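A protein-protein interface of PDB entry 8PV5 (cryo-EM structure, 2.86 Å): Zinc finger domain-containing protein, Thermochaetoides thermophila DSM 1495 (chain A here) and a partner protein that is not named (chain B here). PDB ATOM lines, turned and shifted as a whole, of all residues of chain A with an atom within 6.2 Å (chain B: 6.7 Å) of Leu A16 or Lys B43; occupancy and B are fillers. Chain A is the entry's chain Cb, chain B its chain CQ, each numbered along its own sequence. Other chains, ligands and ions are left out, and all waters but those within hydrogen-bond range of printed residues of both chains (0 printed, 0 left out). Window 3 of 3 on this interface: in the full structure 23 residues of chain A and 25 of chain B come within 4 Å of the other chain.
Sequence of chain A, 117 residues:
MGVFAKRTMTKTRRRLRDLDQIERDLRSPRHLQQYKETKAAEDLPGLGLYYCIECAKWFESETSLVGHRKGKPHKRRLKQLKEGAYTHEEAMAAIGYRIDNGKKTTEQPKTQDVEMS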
ATOM      1  N   THR A  12      25.380 -26.102  16.092  1.00  0.00           N
ATOM      2  CA  THR A  12      25.867 -24.777  15.720  1.00  0.00           C
ATOM      3  C   THR A  12      26.346 -24.741  14.272  1.00  0.00           C
ATOM      4  O   THR A  12      26.176 -23.727  13.586  1.00  0.00           O
ATOM      5  CB  THR A  12      26.989 -24.352  16.670  1.00  0.00           C
ATOM      6  OG1 THR A  12      26.558 -24.532  18.024  1.00  0.00           O
ATOM      7  CG2 THR A  12      27.348 -22.891  16.468  1.00  0.00           C
ATOM      8  N   ARG A  14      25.018 -26.242  11.840  1.00  0.00           N
ATOM      9  CA  ARG A  14      23.845 -26.244  10.975  1.00  0.00           C
ATOM     10  C   ARG A  14      22.968 -25.017  11.187  1.00  0.00           C
ATOM     11  O   ARG A  14      21.800 -25.026  10.792  1.00  0.00           O
ATOM     12  CB  ARG A  14      23.025 -27.516  11.199  1.00  0.00           C
ATOM     13  CG  ARG A  14      23.739 -28.793  10.806  1.00  0.00           C
ATOM     14  CD  ARG A  14      23.449 -29.161   9.361  1.00  0.00           C
ATOM     15  NE  ARG A  14      22.017 -29.258   9.102  1.00  0.00           N
ATOM     16  CZ  ARG A  14      21.287 -30.340   9.328  1.00  0.00           C
ATOM     17  NH1 ARG A  14      21.819 -31.439   9.836  1.00  0.00           N
ATOM     18  NH2 ARG A  14      19.989 -30.319   9.041  1.00  0.00           N
ATOM     19  N   ARG A  15      23.505 -23.969  11.806  1.00  0.00           N
ATOM     20  CA  ARG A  15      22.719 -22.792  12.145  1.00  0.00           C
ATOM     21  C   ARG A  15      22.378 -21.989  10.893  1.00  0.00           C
ATOM     22  O   ARG A  15      23.168 -21.899   9.950  1.00  0.00           O
ATOM     23  CB  ARG A  15      23.496 -21.925  13.138  1.00  0.00           C
ATOM     24  CG  ARG A  15      22.762 -20.703  13.641  1.00  0.00           C
ATOM     25  CD  ARG A  15      23.590 -19.945  14.649  1.00  0.00           C
ATOM     26  NE  ARG A  15      22.861 -18.793  15.160  1.00  0.00           N
ATOM     27  CZ  ARG A  15      22.893 -17.588  14.611  1.00  0.00           C
ATOM     28  NH1 ARG A  15      23.593 -17.347  13.514  1.00  0.00           N
ATOM     29  NH2 ARG A  15      22.205 -16.602  15.173  1.00  0.00           N
ATOM     30  N   LEU A  16      21.180 -21.406  10.887  1.00  0.00           N
ATOM     31  CA  LEU A  16      20.716 -20.562   9.798  1.00  0.00           C
ATOM     32  C   LEU A  16      20.655 -19.107  10.250  1.00  0.00           C
ATOM     33  O   LEU A  16      20.790 -18.794  11.436  1.00  0.00           O
ATOM     34  CB  LEU A  16      19.340 -21.011   9.292  1.00  0.00           C
ATOM     35  CG  LEU A  16      19.216 -22.478   8.881  1.00  0.00           C
ATOM     36  CD1 LEU A  16      17.804 -22.782   8.409  1.00  0.00           C
ATOM     37  CD2 LEU A  16      20.230 -22.822   7.805  1.00  0.00           C
ATOM     38  N   ARG A  17      20.449 -18.220   9.279  1.00  0.00           N
ATOM     39  CA  ARG A  17      20.420 -16.789   9.545  1.00  0.00           C
ATOM     40  C   ARG A  17      19.150 -16.400  10.299  1.00  0.00           C
ATOM     41  O   ARG A  17      18.083 -16.981  10.092  1.00  0.00           O
ATOM     42  CB  ARG A  17      20.520 -16.021   8.227  1.00  0.00           C
ATOM     43  CG  ARG A  17      20.801 -14.542   8.367  1.00  0.00           C
ATOM     44  CD  ARG A  17      21.379 -13.988   7.083  1.00  0.00           C
ATOM     45  NE  ARG A  17      21.711 -12.575   7.192  1.00  0.00           N
ATOM     46  CZ  ARG A  17      22.820 -12.102   7.745  1.00  0.00           C
ATOM     47  NH1 ARG A  17      23.718 -12.904   8.291  1.00  0.00           N
ATOM     48  NH2 ARG A  17      23.030 -10.792   7.751  1.00  0.00           N
ATOM     49  N   ASP A  18      19.275 -15.407  11.178  1.00  0.00           N
ATOM     50  CA  ASP A  18      18.180 -15.024  12.056  1.00  0.00           C
ATOM     51  C   ASP A  18      17.264 -13.981  11.423  1.00  0.00           C
ATOM     52  O   ASP A  18      17.631 -13.280  10.470  1.00  0.00           O
ATOM     53  CB  ASP A  18      18.715 -14.488  13.382  1.00  0.00           C
ATOM     54  CG  ASP A  18      19.364 -15.558  14.225  1.00  0.00           C
ATOM     55  OD1 ASP A  18      18.957 -16.731  14.110  1.00  0.00           O
ATOM     56  OD2 ASP A  18      20.274 -15.228  15.012  1.00  0.00           O
ATOM     57  N   GLN A  21      18.479 -10.333  11.708  1.00  0.00           N
ATOM     58  CA  GLN A  21      19.526 -10.100  10.717  1.00  0.00           C
ATOM     59  C   GLN A  21      18.940  -9.948   9.320  1.00  0.00           C
ATOM     60  O   GLN A  21      19.427  -9.137   8.523  1.00  0.00           O
ATOM     61  CB  GLN A  21      20.546 -11.237  10.752  1.00  0.00           C
ATOM     62  CG  GLN A  21      21.264 -11.383  12.081  1.00  0.00           C
ATOM     63  CD  GLN A  21      22.225 -12.551  12.097  1.00  0.00           C
ATOM     64  OE1 GLN A  21      21.814 -13.708  12.156  1.00  0.00           O
ATOM     65  NE2 GLN A  21      23.517 -12.254  12.035  1.00  0.00           N
ATOM     66  N   ARG A  77       7.864 -16.801   6.375  1.00  0.00           N
ATOM     67  CA  ARG A  77       8.888 -15.784   6.585  1.00  0.00           C
ATOM     68  C   ARG A  77       8.326 -14.382   6.380  1.00  0.00           C
ATOM     69  O   ARG A  77       8.647 -13.464   7.141  1.00  0.00           O
ATOM     70  CB  ARG A  77      10.077 -16.032   5.659  1.00  0.00           C
ATOM     71  CG  ARG A  77      11.092 -17.011   6.225  1.00  0.00           C
ATOM     72  CD  ARG A  77      11.725 -16.475   7.497  1.00  0.00           C
ATOM     73  NE  ARG A  77      12.446 -17.509   8.230  1.00  0.00           N
ATOM     74  CZ  ARG A  77      13.711 -17.841   8.012  1.00  0.00           C
ATOM     75  NH1 ARG A  77      14.440 -17.222   7.099  1.00  0.00           N
ATOM     76  NH2 ARG A  77      14.258 -18.816   8.730  1.00  0.00           N
ATOM     77  N   GLN A  80       6.217 -13.545   9.458  1.00  0.00           N
ATOM     78  CA  GLN A  80       7.071 -13.244  10.604  1.00  0.00           C
ATOM     79  C   GLN A  80       7.731 -11.877  10.458  1.00  0.00           C
ATOM     80  O   GLN A  80       7.896 -11.152  11.446  1.00  0.00           O
ATOM     81  CB  GLN A  80       8.122 -14.339  10.768  1.00  0.00           C
ATOM     82  CG  GLN A  80       7.578 -15.617  11.381  1.00  0.00           C
ATOM     83  CD  GLN A  80       8.587 -16.744  11.374  1.00  0.00           C
ATOM     84  OE1 GLN A  80       9.626 -16.656  10.723  1.00  0.00           O
ATOM     85  NE2 GLN A  80       8.285 -17.812  12.099  1.00  0.00           N
ATOM     86  N   PHE B   8      15.551 -13.801  26.333  1.00  0.00           N
ATOM     87  CA  PHE B   8      14.372 -14.524  25.875  1.00  0.00           C
ATOM     88  C   PHE B   8      13.164 -14.268  26.769  1.00  0.00           C
ATOM     89  O   PHE B   8      12.096 -13.883  26.282  1.00  0.00           O
ATOM     90  CB  PHE B   8      14.685 -16.018  25.803  1.00  0.00           C
ATOM     91  CG  PHE B   8      13.869 -16.758  24.788  1.00  0.00           C
ATOM     92  CD1 PHE B   8      12.655 -17.323  25.135  1.00  0.00           C
ATOM     93  CD2 PHE B   8      14.315 -16.885  23.484  1.00  0.00           C
ATOM     94  CE1 PHE B   8      11.902 -18.000  24.204  1.00  0.00           C
ATOM     95  CE2 PHE B   8      13.567 -17.565  22.549  1.00  0.00           C
ATOM     96  CZ  PHE B   8      12.357 -18.119  22.910  1.00  0.00           C
ATOM     97  N   LYS B  38      17.662 -23.176  24.283  1.00  0.00           N
ATOM     98  CA  LYS B  38      17.217 -24.152  23.296  1.00  0.00           C
ATOM     99  C   LYS B  38      16.038 -23.630  22.486  1.00  0.00           C
ATOM    100  O   LYS B  38      15.924 -23.930  21.293  1.00  0.00           O
ATOM    101  CB  LYS B  38      16.862 -25.466  23.985  1.00  0.00           C
ATOM    102  CG  LYS B  38      18.069 -26.258  24.449  1.00  0.00           C
ATOM    103  CD  LYS B  38      17.654 -27.492  25.220  1.00  0.00           C
ATOM    104  CE  LYS B  38      18.863 -28.276  25.693  1.00  0.00           C
ATOM    105  NZ  LYS B  38      18.467 -29.558  26.334  1.00  0.00           N
ATOM    106  N   ASN B  39      15.157 -22.841  23.106  1.00  0.00           N
ATOM    107  CA  ASN B  39      14.075 -22.226  22.344  1.00  0.00           C
ATOM    108  C   ASN B  39      14.613 -21.199  21.352  1.00  0.00           C
ATOM    109  O   ASN B  39      14.120 -21.099  20.219  1.00  0.00           O
ATOM    110  CB  ASN B  39      13.063 -21.595  23.295  1.00  0.00           C
ATOM    111  CG  ASN B  39      12.139 -22.618  23.917  1.00  0.00           C
ATOM    112  OD1 ASN B  39      11.456 -23.360  23.215  1.00  0.00           O
ATOM    113  ND2 ASN B  39      12.123 -22.671  25.241  1.00  0.00           N
ATOM    114  N   PHE B  40      15.641 -20.441  21.751  1.00  0.00           N
ATOM    115  CA  PHE B  40      16.293 -19.522  20.823  1.00  0.00           C
ATOM    116  C   PHE B  40      16.953 -20.273  19.671  1.00  0.00           C
ATOM    117  O   PHE B  40      16.876 -19.839  18.516  1.00  0.00           O
ATOM    118  CB  PHE B  40      17.319 -18.668  21.572  1.00  0.00           C
ATOM    119  CG  PHE B  40      18.012 -17.646  20.710  1.00  0.00           C
ATOM    120  CD1 PHE B  40      17.429 -16.414  20.476  1.00  0.00           C
ATOM    121  CD2 PHE B  40      19.254 -17.910  20.151  1.00  0.00           C
ATOM    122  CE1 PHE B  40      18.062 -15.471  19.691  1.00  0.00           C
ATOM    123  CE2 PHE B  40      19.887 -16.973  19.364  1.00  0.00           C
ATOM    124  CZ  PHE B  40      19.292 -15.753  19.135  1.00  0.00           C
ATOM    125  N   LYS B  41      17.608 -21.400  19.966  1.00  0.00           N
ATOM    126  CA  LYS B  41      18.223 -22.202  18.914  1.00  0.00           C
ATOM    127  C   LYS B  41      17.196 -22.853  17.997  1.00  0.00           C
ATOM    128  O   LYS B  41      17.481 -23.050  16.811  1.00  0.00           O
ATOM    129  CB  LYS B  41      19.129 -23.274  19.519  1.00  0.00           C
ATOM    130  CG  LYS B  41      20.366 -22.719  20.190  1.00  0.00           C
ATOM    131  CD  LYS B  41      21.029 -23.760  21.063  1.00  0.00           C
ATOM    132  CE  LYS B  41      21.523 -24.930  20.243  1.00  0.00           C
ATOM    133  NZ  LYS B  41      22.641 -24.531  19.344  1.00  0.00           N
ATOM    134  N   MET B  42      16.014 -23.187  18.511  1.00  0.00           N
ATOM    135  CA  MET B  42      14.910 -23.648  17.681  1.00  0.00           C
ATOM    136  C   MET B  42      14.143 -22.501  17.043  1.00  0.00           C
ATOM    137  O   MET B  42      13.157 -22.755  16.346  1.00  0.00           O
ATOM    138  CB  MET B  42      13.943 -24.512  18.494  1.00  0.00           C
ATOM    139  CG  MET B  42      14.518 -25.831  18.968  1.00  0.00           C
ATOM    140  SD  MET B  42      13.300 -26.816  19.855  1.00  0.00           S
ATOM    141  CE  MET B  42      13.207 -25.928  21.405  1.00  0.00           C
ATOM    142  N   LYS B  43      14.563 -21.254  17.291  1.00  0.00           N
ATOM    143  CA  LYS B  43      14.024 -20.047  16.650  1.00  0.00           C
ATOM    144  C   LYS B  43      12.563 -19.817  17.033  1.00  0.00           C
ATOM    145  O   LYS B  43      11.788 -19.256  16.259  1.00  0.00           O
ATOM    146  CB  LYS B  43      14.180 -20.065  15.122  1.00  0.00           C
ATOM    147  CG  LYS B  43      15.511 -20.579  14.584  1.00  0.00           C
ATOM    148  CD  LYS B  43      16.630 -19.567  14.702  1.00  0.00           C
ATOM    149  CE  LYS B  43      17.876 -20.087  14.003  1.00  0.00           C
ATOM    150  NZ  LYS B  43      18.961 -19.077  13.934  1.00  0.00           N
ATOM    151  N   ARG B  44      12.185 -20.258  18.227  1.00  0.00           N
ATOM    152  CA  ARG B  44      10.875 -19.929  18.765  1.00  0.00           C
ATOM    153  C   ARG B  44      10.843 -18.461  19.164  1.00  0.00           C
ATOM    154  O   ARG B  44      11.776 -17.951  19.788  1.00  0.00           O
ATOM    155  CB  ARG B  44      10.547 -20.815  19.966  1.00  0.00           C
ATOM    156  CG  ARG B  44      10.660 -22.301  19.685  1.00  0.00           C
ATOM    157  CD  ARG B  44       9.567 -23.082  20.391  1.00  0.00           C
ATOM    158  NE  ARG B  44       8.262 -22.869  19.780  1.00  0.00           N
ATOM    159  CZ  ARG B  44       7.124 -23.356  20.254  1.00  0.00           C
ATOM    160  NH1 ARG B  44       7.093 -24.092  21.353  1.00  0.00           N
ATOM    161  NH2 ARG B  44       5.989 -23.096  19.612  1.00  0.00           N
ATOM    162  N   ASN B  45       9.770 -17.778  18.784  1.00  0.00           N
ATOM    163  CA  ASN B  45       9.661 -16.347  19.025  1.00  0.00           C
ATOM    164  C   ASN B  45       9.211 -16.104  20.459  1.00  0.00           C
ATOM    165  O   ASN B  45       8.200 -16.681  20.882  1.00  0.00           O
ATOM    166  CB  ASN B  45       8.684 -15.719  18.050  1.00  0.00           C
ATOM    167  CG  ASN B  45       8.876 -14.227  17.918  1.00  0.00           C
ATOM    168  OD1 ASN B  45       9.846 -13.767  17.320  1.00  0.00           O
ATOM    169  ND2 ASN B  45       7.944 -13.464  18.460  1.00  0.00           N
ATOM    170  N   PRO B  46       9.936 -15.298  21.244  1.00  0.00           N
ATOM    171  CA  PRO B  46       9.528 -15.069  22.642  1.00  0.00           C
ATOM    172  C   PRO B  46       8.199 -14.350  22.787  1.00  0.00           C
ATOM    173  O   PRO B  46       7.515 -14.521  23.803  1.00  0.00           O
ATOM    174  CB  PRO B  46      10.683 -14.228  23.203  1.00  0.00           C
ATOM    175  CG  PRO B  46      11.826 -14.487  22.301  1.00  0.00           C
ATOM    176  CD  PRO B  46      11.240 -14.689  20.943  1.00  0.00           C
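The guanidinium group (NH2) of Arg A15 lies within salt-bridge range of the side-chain carboxylate (OD1) of Asp A18, 3.4 Å away. N of Asp A18 sits at hydrogen-bond distance from OE1 of Gln A21 (3.2 Å).
The side-chain amino group (NZ) of Lys B43 is in hydrogen-bond range of the backbone carbonyl oxygen (O) of Leu A16. OD1 of Asp A18 sits close to NZ of Lys B43, 2.4 Å away.
Printed residues of chain B that touch a printed residue of chain A: Lys B43. Among the printed residues, Asp or Glu carboxylates within 4 Å of a Lys or Arg side-chain nitrogen of the other chain: Asp A18 with Lys B43 (2.4 Å).
Leu A16 touches just one residue of chain B: Lys B43. Of the printed residues of chain B, Asp A18 touches Lys B43 (2.4 Å).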
